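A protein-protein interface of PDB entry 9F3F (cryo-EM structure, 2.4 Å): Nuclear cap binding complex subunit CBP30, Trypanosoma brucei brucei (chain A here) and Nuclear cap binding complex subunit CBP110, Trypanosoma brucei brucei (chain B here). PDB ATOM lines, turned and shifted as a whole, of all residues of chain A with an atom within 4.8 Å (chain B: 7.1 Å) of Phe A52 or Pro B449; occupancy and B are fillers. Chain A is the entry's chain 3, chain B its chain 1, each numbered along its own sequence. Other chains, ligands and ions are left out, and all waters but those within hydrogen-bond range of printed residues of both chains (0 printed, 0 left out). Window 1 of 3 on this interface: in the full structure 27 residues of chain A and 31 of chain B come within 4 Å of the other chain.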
ATOM      1  N   TRP A  48      13.938  24.419   4.252  1.00  0.00           N
ATOM      2  CA  TRP A  48      13.905  23.210   5.111  1.00  0.00           C
ATOM      3  C   TRP A  48      14.816  22.133   4.540  1.00  0.00           C
ATOM      4  O   TRP A  48      15.480  21.453   5.335  1.00  0.00           O
ATOM      5  CB  TRP A  48      12.468  22.723   5.308  1.00  0.00           C
ATOM      6  CG  TRP A  48      11.714  23.481   6.366  1.00  0.00           C
ATOM      7  CD1 TRP A  48      10.852  24.518   6.183  1.00  0.00           C
ATOM      8  CD2 TRP A  48      11.772  23.250   7.787  1.00  0.00           C
ATOM      9  NE1 TRP A  48      10.364  24.944   7.386  1.00  0.00           N
ATOM     10  CE2 TRP A  48      10.908  24.187   8.388  1.00  0.00           C
ATOM     11  CE3 TRP A  48      12.454  22.343   8.603  1.00  0.00           C
ATOM     12  CZ2 TRP A  48      10.718  24.244   9.765  1.00  0.00           C
ATOM     13  CZ3 TRP A  48      12.264  22.401   9.963  1.00  0.00           C
ATOM     14  CH2 TRP A  48      11.408  23.338  10.534  1.00  0.00           C
ATOM     15  N   ARG A  49      14.874  21.999   3.220  1.00  0.00           N
ATOM     16  CA  ARG A  49      15.841  21.075   2.635  1.00  0.00           C
ATOM     17  C   ARG A  49      17.263  21.485   2.988  1.00  0.00           C
ATOM     18  O   ARG A  49      18.099  20.638   3.327  1.00  0.00           O
ATOM     19  CB  ARG A  49      15.666  21.016   1.122  1.00  0.00           C
ATOM     20  CG  ARG A  49      14.320  20.508   0.683  1.00  0.00           C
ATOM     21  CD  ARG A  49      14.451  19.359  -0.281  1.00  0.00           C
ATOM     22  NE  ARG A  49      13.158  18.979  -0.832  1.00  0.00           N
ATOM     23  CZ  ARG A  49      12.514  19.664  -1.765  1.00  0.00           C
ATOM     24  NH1 ARG A  49      13.031  20.756  -2.299  1.00  0.00           N
ATOM     25  NH2 ARG A  49      11.327  19.234  -2.180  1.00  0.00           N
ATOM     26  N   SER A  50      17.553  22.784   2.919  1.00  0.00           N
ATOM     27  CA  SER A  50      18.868  23.268   3.313  1.00  0.00           C
ATOM     28  C   SER A  50      19.129  23.000   4.786  1.00  0.00           C
ATOM     29  O   SER A  50      20.249  22.658   5.169  1.00  0.00           O
ATOM     30  CB  SER A  50      18.989  24.758   3.007  1.00  0.00           C
ATOM     31  OG  SER A  50      18.596  25.032   1.674  1.00  0.00           O
ATOM     32  N   ALA A  51      18.109  23.152   5.628  1.00  0.00           N
ATOM     33  CA  ALA A  51      18.274  22.881   7.051  1.00  0.00           C
ATOM     34  C   ALA A  51      18.547  21.407   7.310  1.00  0.00           C
ATOM     35  O   ALA A  51      19.366  21.063   8.165  1.00  0.00           O
ATOM     36  CB  ALA A  51      17.037  23.335   7.817  1.00  0.00           C
ATOM     37  N   PHE A  52      17.852  20.519   6.594  1.00  0.00           N
ATOM     38  CA  PHE A  52      18.136  19.093   6.708  1.00  0.00           C
ATOM     39  C   PHE A  52      19.565  18.791   6.285  1.00  0.00           C
ATOM     40  O   PHE A  52      20.278  18.031   6.955  1.00  0.00           O
ATOM     41  CB  PHE A  52      17.157  18.288   5.855  1.00  0.00           C
ATOM     42  CG  PHE A  52      15.721  18.457   6.245  1.00  0.00           C
ATOM     43  CD1 PHE A  52      15.368  18.729   7.552  1.00  0.00           C
ATOM     44  CD2 PHE A  52      14.720  18.332   5.300  1.00  0.00           C
ATOM     45  CE1 PHE A  52      14.047  18.881   7.905  1.00  0.00           C
ATOM     46  CE2 PHE A  52      13.398  18.484   5.649  1.00  0.00           C
ATOM     47  CZ  PHE A  52      13.062  18.759   6.954  1.00  0.00           C
ATOM     48  N   SER A  53      19.997  19.384   5.170  1.00  0.00           N
ATOM     49  CA  SER A  53      21.358  19.176   4.694  1.00  0.00           C
ATOM     50  C   SER A  53      22.377  19.665   5.712  1.00  0.00           C
ATOM     51  O   SER A  53      23.379  18.991   5.968  1.00  0.00           O
ATOM     52  CB  SER A  53      21.555  19.886   3.358  1.00  0.00           C
ATOM     53  OG  SER A  53      21.106  19.080   2.285  1.00  0.00           O
ATOM     54  N   GLN A  54      22.140  20.835   6.303  1.00  0.00           N
ATOM     55  CA  GLN A  54      23.067  21.364   7.296  1.00  0.00           C
ATOM     56  C   GLN A  54      23.070  20.517   8.559  1.00  0.00           C
ATOM     57  O   GLN A  54      24.125  20.308   9.163  1.00  0.00           O
ATOM     58  CB  GLN A  54      22.726  22.817   7.621  1.00  0.00           C
ATOM     59  CG  GLN A  54      22.818  23.758   6.432  1.00  0.00           C
ATOM     60  CD  GLN A  54      22.241  25.126   6.720  1.00  0.00           C
ATOM     61  OE1 GLN A  54      21.776  25.394   7.825  1.00  0.00           O
ATOM     62  NE2 GLN A  54      22.268  26.001   5.723  1.00  0.00           N
ATOM     63  N   TYR A  55      21.905  20.021   8.976  1.00  0.00           N
ATOM     64  CA  TYR A  55      21.853  19.180  10.164  1.00  0.00           C
ATOM     65  C   TYR A  55      22.608  17.879   9.950  1.00  0.00           C
ATOM     66  O   TYR A  55      23.288  17.393  10.858  1.00  0.00           O
ATOM     67  CB  TYR A  55      20.406  18.887  10.560  1.00  0.00           C
ATOM     68  CG  TYR A  55      20.330  17.957  11.742  1.00  0.00           C
ATOM     69  CD1 TYR A  55      20.646  18.406  13.008  1.00  0.00           C
ATOM     70  CD2 TYR A  55      19.987  16.626  11.588  1.00  0.00           C
ATOM     71  CE1 TYR A  55      20.608  17.565  14.090  1.00  0.00           C
ATOM     72  CE2 TYR A  55      19.947  15.775  12.669  1.00  0.00           C
ATOM     73  CZ  TYR A  55      20.258  16.253  13.919  1.00  0.00           C
ATOM     74  OH  TYR A  55      20.222  15.425  15.011  1.00  0.00           O
ATOM     75  N   THR A  56      22.484  17.287   8.763  1.00  0.00           N
ATOM     76  CA  THR A  56      23.213  16.052   8.495  1.00  0.00           C
ATOM     77  C   THR A  56      24.700  16.310   8.300  1.00  0.00           C
ATOM     78  O   THR A  56      25.526  15.470   8.677  1.00  0.00           O
ATOM     79  CB  THR A  56      22.634  15.351   7.270  1.00  0.00           C
ATOM     80  OG1 THR A  56      22.524  16.285   6.190  1.00  0.00           O
ATOM     81  CG2 THR A  56      21.260  14.797   7.584  1.00  0.00           C
ATOM     82  N   SER B 380      17.214  29.038   7.649  1.00  0.00           N
ATOM     83  CA  SER B 380      17.800  27.705   7.659  1.00  0.00           C
ATOM     84  C   SER B 380      18.371  27.365   9.026  1.00  0.00           C
ATOM     85  O   SER B 380      18.291  26.217   9.466  1.00  0.00           O
ATOM     86  CB  SER B 380      18.882  27.601   6.587  1.00  0.00           C
ATOM     87  OG  SER B 380      18.460  28.207   5.378  1.00  0.00           O
ATOM     88  N   ALA B 383      15.528  26.570  11.465  1.00  0.00           N
ATOM     89  CA  ALA B 383      15.024  25.250  11.050  1.00  0.00           C
ATOM     90  C   ALA B 383      15.970  24.149  11.525  1.00  0.00           C
ATOM     91  O   ALA B 383      15.491  23.049  11.843  1.00  0.00           O
ATOM     92  CB  ALA B 383      14.875  25.265   9.565  1.00  0.00           C
ATOM     93  N   ASN B 384      17.262  24.444  11.610  1.00  0.00           N
ATOM     94  CA  ASN B 384      18.280  23.446  12.023  1.00  0.00           C
ATOM     95  C   ASN B 384      18.103  23.144  13.512  1.00  0.00           C
ATOM     96  O   ASN B 384      18.169  21.959  13.870  1.00  0.00           O
ATOM     97  CB  ASN B 384      19.674  23.872  11.563  1.00  0.00           C
ATOM     98  CG  ASN B 384      20.766  22.902  11.934  1.00  0.00           C
ATOM     99  OD1 ASN B 384      21.035  22.681  13.118  1.00  0.00           O
ATOM    100  ND2 ASN B 384      21.426  22.340  10.933  1.00  0.00           N
ATOM    101  N   VAL B 387      14.980  21.040  14.046  1.00  0.00           N
ATOM    102  CA  VAL B 387      15.256  19.609  13.715  1.00  0.00           C
ATOM    103  C   VAL B 387      16.135  19.004  14.820  1.00  0.00           C
ATOM    104  O   VAL B 387      15.768  17.928  15.339  1.00  0.00           O
ATOM    105  CB  VAL B 387      15.928  19.468  12.335  1.00  0.00           C
ATOM    106  CG1 VAL B 387      16.395  18.042  12.069  1.00  0.00           C
ATOM    107  CG2 VAL B 387      15.022  19.955  11.212  1.00  0.00           C
ATOM    108  N   GLN B 391      15.341  15.741  16.873  1.00  0.00           N
ATOM    109  CA  GLN B 391      16.190  14.562  16.809  1.00  0.00           C
ATOM    110  C   GLN B 391      16.772  14.219  18.168  1.00  0.00           C
ATOM    111  O   GLN B 391      16.951  13.040  18.478  1.00  0.00           O
ATOM    112  CB  GLN B 391      17.306  14.775  15.795  1.00  0.00           C
ATOM    113  CG  GLN B 391      16.840  14.799  14.360  1.00  0.00           C
ATOM    114  CD  GLN B 391      16.473  13.429  13.846  1.00  0.00           C
ATOM    115  OE1 GLN B 391      15.585  13.287  13.007  1.00  0.00           O
ATOM    116  NE2 GLN B 391      17.152  12.410  14.346  1.00  0.00           N
ATOM    117  N   LEU B 441       6.051  17.525  10.166  1.00  0.00           N
ATOM    118  CA  LEU B 441       6.427  16.869   8.921  1.00  0.00           C
ATOM    119  C   LEU B 441       5.435  17.178   7.816  1.00  0.00           C
ATOM    120  O   LEU B 441       5.830  17.390   6.664  1.00  0.00           O
ATOM    121  CB  LEU B 441       6.546  15.361   9.121  1.00  0.00           C
ATOM    122  CG  LEU B 441       7.860  14.871   9.720  1.00  0.00           C
ATOM    123  CD1 LEU B 441       7.619  13.621  10.533  1.00  0.00           C
ATOM    124  CD2 LEU B 441       8.884  14.627   8.631  1.00  0.00           C
ATOM    125  N   VAL B 444       6.351  20.409   6.415  1.00  0.00           N
ATOM    126  CA  VAL B 444       7.564  20.395   5.611  1.00  0.00           C
ATOM    127  C   VAL B 444       7.510  19.313   4.529  1.00  0.00           C
ATOM    128  O   VAL B 444       8.550  18.825   4.094  1.00  0.00           O
ATOM    129  CB  VAL B 444       8.818  20.252   6.484  1.00  0.00           C
ATOM    130  CG1 VAL B 444       8.886  21.387   7.479  1.00  0.00           C
ATOM    131  CG2 VAL B 444       8.823  18.925   7.206  1.00  0.00           C
ATOM    132  N   PHE B 446       6.707  16.214   4.622  1.00  0.00           N
ATOM    133  CA  PHE B 446       7.094  14.848   5.075  1.00  0.00           C
ATOM    134  C   PHE B 446       8.557  14.572   4.736  1.00  0.00           C
ATOM    135  O   PHE B 446       8.911  13.401   4.541  1.00  0.00           O
ATOM    136  CB  PHE B 446       6.106  13.820   4.525  1.00  0.00           C
ATOM    137  CG  PHE B 446       4.683  13.971   4.994  1.00  0.00           C
ATOM    138  CD1 PHE B 446       4.363  13.863   6.335  1.00  0.00           C
ATOM    139  CD2 PHE B 446       3.669  14.251   4.095  1.00  0.00           C
ATOM    140  CE1 PHE B 446       3.053  13.999   6.762  1.00  0.00           C
ATOM    141  CE2 PHE B 446       2.363  14.400   4.526  1.00  0.00           C
ATOM    142  CZ  PHE B 446       2.056  14.269   5.857  1.00  0.00           C
ATOM    143  N   GLU B 447       9.380  15.617   4.707  1.00  0.00           N
ATOM    144  CA  GLU B 447      10.820  15.478   4.397  1.00  0.00           C
ATOM    145  C   GLU B 447      11.564  15.666   5.709  1.00  0.00           C
ATOM    146  O   GLU B 447      11.175  16.554   6.470  1.00  0.00           O
ATOM    147  CB  GLU B 447      11.223  16.461   3.301  1.00  0.00           C
ATOM    148  CG  GLU B 447      10.456  16.253   2.011  1.00  0.00           C
ATOM    149  CD  GLU B 447      10.851  17.182   0.880  1.00  0.00           C
ATOM    150  OE1 GLU B 447      11.748  18.014   1.092  1.00  0.00           O
ATOM    151  OE2 GLU B 447      10.267  17.066  -0.212  1.00  0.00           O
ATOM    152  N   TRP B 448      12.534  14.810   5.987  1.00  0.00           N
ATOM    153  CA  TRP B 448      13.271  14.861   7.263  1.00  0.00           C
ATOM    154  C   TRP B 448      14.617  14.195   6.995  1.00  0.00           C
ATOM    155  O   TRP B 448      14.761  13.606   5.917  1.00  0.00           O
ATOM    156  CB  TRP B 448      12.473  14.089   8.315  1.00  0.00           C
ATOM    157  CG  TRP B 448      12.801  14.380   9.741  1.00  0.00           C
ATOM    158  CD1 TRP B 448      13.273  13.508  10.673  1.00  0.00           C
ATOM    159  CD2 TRP B 448      12.598  15.630  10.419  1.00  0.00           C
ATOM    160  NE1 TRP B 448      13.413  14.143  11.875  1.00  0.00           N
ATOM    161  CE2 TRP B 448      13.010  15.444  11.752  1.00  0.00           C
ATOM    162  CE3 TRP B 448      12.127  16.887  10.029  1.00  0.00           C
ATOM    163  CZ2 TRP B 448      12.965  16.468  12.692  1.00  0.00           C
ATOM    164  CZ3 TRP B 448      12.081  17.900  10.959  1.00  0.00           C
ATOM    165  CH2 TRP B 448      12.496  17.690  12.272  1.00  0.00           C
ATOM    166  N   PRO B 449      15.611  14.252   7.899  1.00  0.00           N
ATOM    167  CA  PRO B 449      16.817  13.464   7.723  1.00  0.00           C
ATOM    168  C   PRO B 449      16.444  12.018   8.071  1.00  0.00           C
ATOM    169  O   PRO B 449      16.871  11.548   9.095  1.00  0.00           O
ATOM    170  CB  PRO B 449      17.690  14.003   8.851  1.00  0.00           C
ATOM    171  CG  PRO B 449      17.175  15.382   9.122  1.00  0.00           C
ATOM    172  CD  PRO B 449      15.686  15.192   9.014  1.00  0.00           C
ATOM    173  N   TRP B 450      15.647  11.354   7.224  1.00  0.00           N
ATOM    174  CA  TRP B 450      15.109   9.995   7.532  1.00  0.00           C
ATOM    175  C   TRP B 450      16.145   8.874   7.655  1.00  0.00           C
ATOM    176  O   TRP B 450      16.116   8.176   8.679  1.00  0.00           O
ATOM    177  CB  TRP B 450      14.091   9.610   6.458  1.00  0.00           C
ATOM    178  CG  TRP B 450      12.787  10.340   6.498  1.00  0.00           C
ATOM    179  CD1 TRP B 450      12.246  11.126   5.524  1.00  0.00           C
ATOM    180  CD2 TRP B 450      11.820  10.290   7.558  1.00  0.00           C
ATOM    181  NE1 TRP B 450      11.022  11.591   5.918  1.00  0.00           N
ATOM    182  CE2 TRP B 450      10.734  11.093   7.160  1.00  0.00           C
ATOM    183  CE3 TRP B 450      11.772   9.656   8.804  1.00  0.00           C
ATOM    184  CZ2 TRP B 450       9.615  11.276   7.967  1.00  0.00           C
ATOM    185  CZ3 TRP B 450      10.668   9.841   9.601  1.00  0.00           C
ATOM    186  CH2 TRP B 450       9.606  10.640   9.185  1.00  0.00           C
ATOM    187  N   SER B 451      17.033   8.718   6.674  1.00  0.00           N
ATOM    188  CA  SER B 451      18.022   7.614   6.675  1.00  0.00           C
ATOM    189  C   SER B 451      19.015   7.786   7.816  1.00  0.00           C
ATOM    190  O   SER B 451      19.368   6.788   8.442  1.00  0.00           O
ATOM    191  CB  SER B 451      18.699   7.568   5.367  1.00  0.00           C
ATOM    192  OG  SER B 451      19.301   8.817   5.086  1.00  0.00           O
ATOM    193  N   GLU B 452      19.410   9.019   8.074  1.00  0.00           N
ATOM    194  CA  GLU B 452      20.419   9.298   9.105  1.00  0.00           C
ATOM    195  C   GLU B 452      19.835   8.986  10.472  1.00  0.00           C
ATOM    196  O   GLU B 452      20.508   8.307  11.258  1.00  0.00           O
ATOM    197  CB  GLU B 452      20.839  10.756   9.024  1.00  0.00           C
ATOM    198  CG  GLU B 452      21.338  11.239   7.674  1.00  0.00           C
ATOM    199  CD  GLU B 452      20.309  11.394   6.569  1.00  0.00           C
ATOM    200  OE1 GLU B 452      19.126  11.105   6.814  1.00  0.00           O
ATOM    201  OE2 GLU B 452      20.685  11.871   5.486  1.00  0.00           O
ATOM    202  N   SER B 453      18.629   9.464  10.736  1.00  0.00           N
ATOM    203  CA  SER B 453      17.977   9.274  12.023  1.00  0.00           C
ATOM    204  C   SER B 453      17.759   7.798  12.310  1.00  0.00           C
ATOM    205  O   SER B 453      17.993   7.339  13.432  1.00  0.00           O
ATOM    206  CB  SER B 453      16.652  10.034  12.055  1.00  0.00           C
ATOM    207  OG  SER B 453      15.842   9.690  10.946  1.00  0.00           O
ATOM    208  N   LEU B 454      17.318   7.036  11.306  1.00  0.00           N
ATOM    209  CA  LEU B 454      17.112   5.608  11.512  1.00  0.00           C
ATOM    210  C   LEU B 454      18.423   4.906  11.840  1.00  0.00           C
ATOM    211  O   LEU B 454      18.477   4.084  12.760  1.00  0.00           O
ATOM    212  CB  LEU B 454      16.456   4.983  10.283  1.00  0.00           C
ATOM    213  CG  LEU B 454      15.934   3.562  10.488  1.00  0.00           C
ATOM    214  CD1 LEU B 454      14.973   3.509  11.659  1.00  0.00           C
ATOM    215  CD2 LEU B 454      15.272   3.042   9.232  1.00  0.00           C
ATOM    216  N   PHE B 482       9.924   4.592  15.029  1.00  0.00           N
ATOM    217  CA  PHE B 482       9.670   4.993  13.656  1.00  0.00           C
ATOM    218  C   PHE B 482       8.391   4.374  13.116  1.00  0.00           C
ATOM    219  O   PHE B 482       7.719   4.988  12.283  1.00  0.00           O
ATOM    220  CB  PHE B 482      10.878   4.648  12.792  1.00  0.00           C
ATOM    221  CG  PHE B 482      12.000   5.630  12.933  1.00  0.00           C
ATOM    222  CD1 PHE B 482      12.858   5.565  14.012  1.00  0.00           C
ATOM    223  CD2 PHE B 482      12.173   6.639  12.007  1.00  0.00           C
ATOM    224  CE1 PHE B 482      13.877   6.473  14.155  1.00  0.00           C
ATOM    225  CE2 PHE B 482      13.193   7.548  12.144  1.00  0.00           C
ATOM    226  CZ  PHE B 482      14.047   7.464  13.220  1.00  0.00           C
ATOM    227  N   PHE B 506      13.695   1.948   4.806  1.00  0.00           N
ATOM    228  CA  PHE B 506      12.411   1.947   5.488  1.00  0.00           C
ATOM    229  C   PHE B 506      11.436   0.952   4.881  1.00  0.00           C
ATOM    230  O   PHE B 506      10.240   1.011   5.181  1.00  0.00           O
ATOM    231  CB  PHE B 506      11.805   3.350   5.467  1.00  0.00           C
ATOM    232  CG  PHE B 506      12.360   4.261   6.514  1.00  0.00           C
ATOM    233  CD1 PHE B 506      13.564   4.907   6.318  1.00  0.00           C
ATOM    234  CD2 PHE B 506      11.677   4.478   7.691  1.00  0.00           C
ATOM    235  CE1 PHE B 506      14.077   5.745   7.277  1.00  0.00           C
ATOM    236  CE2 PHE B 506      12.185   5.316   8.654  1.00  0.00           C
ATOM    237  CZ  PHE B 506      13.387   5.951   8.447  1.00  0.00           C
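OE1 of Gln B391 sits at hydrogen-bond distance from NE1 of Trp B448 (2.6 Å). O of Pro B449 lies within hydrogen-bond range of OG of Ser B453 (2.8 Å). OG of Ser B451 is in hydrogen-bond range of OE1 of Glu B452 (2.9 Å). The backbone carbonyl oxygen (O) of Phe A52 is in hydrogen-bond range of the side-chain hydroxyl (OG1) of Thr A56 (2.9 Å). The side-chain hydroxyl (OG1) of Thr A56 sits at hydrogen-bond distance from the backbone carbonyl oxygen (O) of Ser A53, at 2.8 Å.
Phe A52 touches just these residues of chain B: Val B387 (3.6 Å), Glu B447 (2.9 Å), Trp B448 (3.5 Å) and Pro B449 (3.8 Å). Of the printed residues of chain B, Thr A56 touches Pro B449 (3.9 Å) and Glu B452 (3.6 Å). Printed residues of chain A within 4 Å of Asn B384: Ala A51, Gln A54 and Tyr A55. Pro B449 touches just these residues of chain A: Phe A52 (3.8 Å), Tyr A55 (3.9 Å) and Thr A56 (3.9 Å). Ser B453 touches none of the printed residues of chain A. Phe B506 touches none of the printed residues of chain A. The nearest residue of chain B that does not touch Phe A52 is Val B444 (4.2 Å). The nearest printed residue of chain A that does not touch Pro B449 is Ala A51 (6.2 Å). The nearest printed residue of chain A that does not touch Ser B380 is Ser A50 (4.2 Å).
ND2 of Asn B384 sits close to N of Tyr A55 (3.1 Å). OE1 of Glu B447 lies within salt-bridge range of NE of Arg A49 (2.6 Å).
CG1 of Val B444 touches CD2 of Trp A48 (3.4 Å). Ala A51 touches Ala B383 (CB to CB, 3.4 Å). O of Ala A51 touches ND2 of Asn B384, 3.7 Å away. Phe A52 touches Val B387 (CE1 to CG2, 3.6 Å). Phe A52 touches Glu B447. CE1 of Phe A52 touches CE3 of Trp B448, at 3.5 Å. Pro B449 touches Phe A52. Asn B384 touches Gln A54 (ND2 to C, 3.4 Å). Thr A56 touches Pro B449. Thr A56 touches Glu B452.
Of the 9 printed residues of chain A, 7 touch a printed residue of chain B. Among the printed residues, Asp or Glu carboxylates within 4 Å of a Lys or Arg side-chain nitrogen of the other chain: Arg A49 with Glu B447 (2.6 Å).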
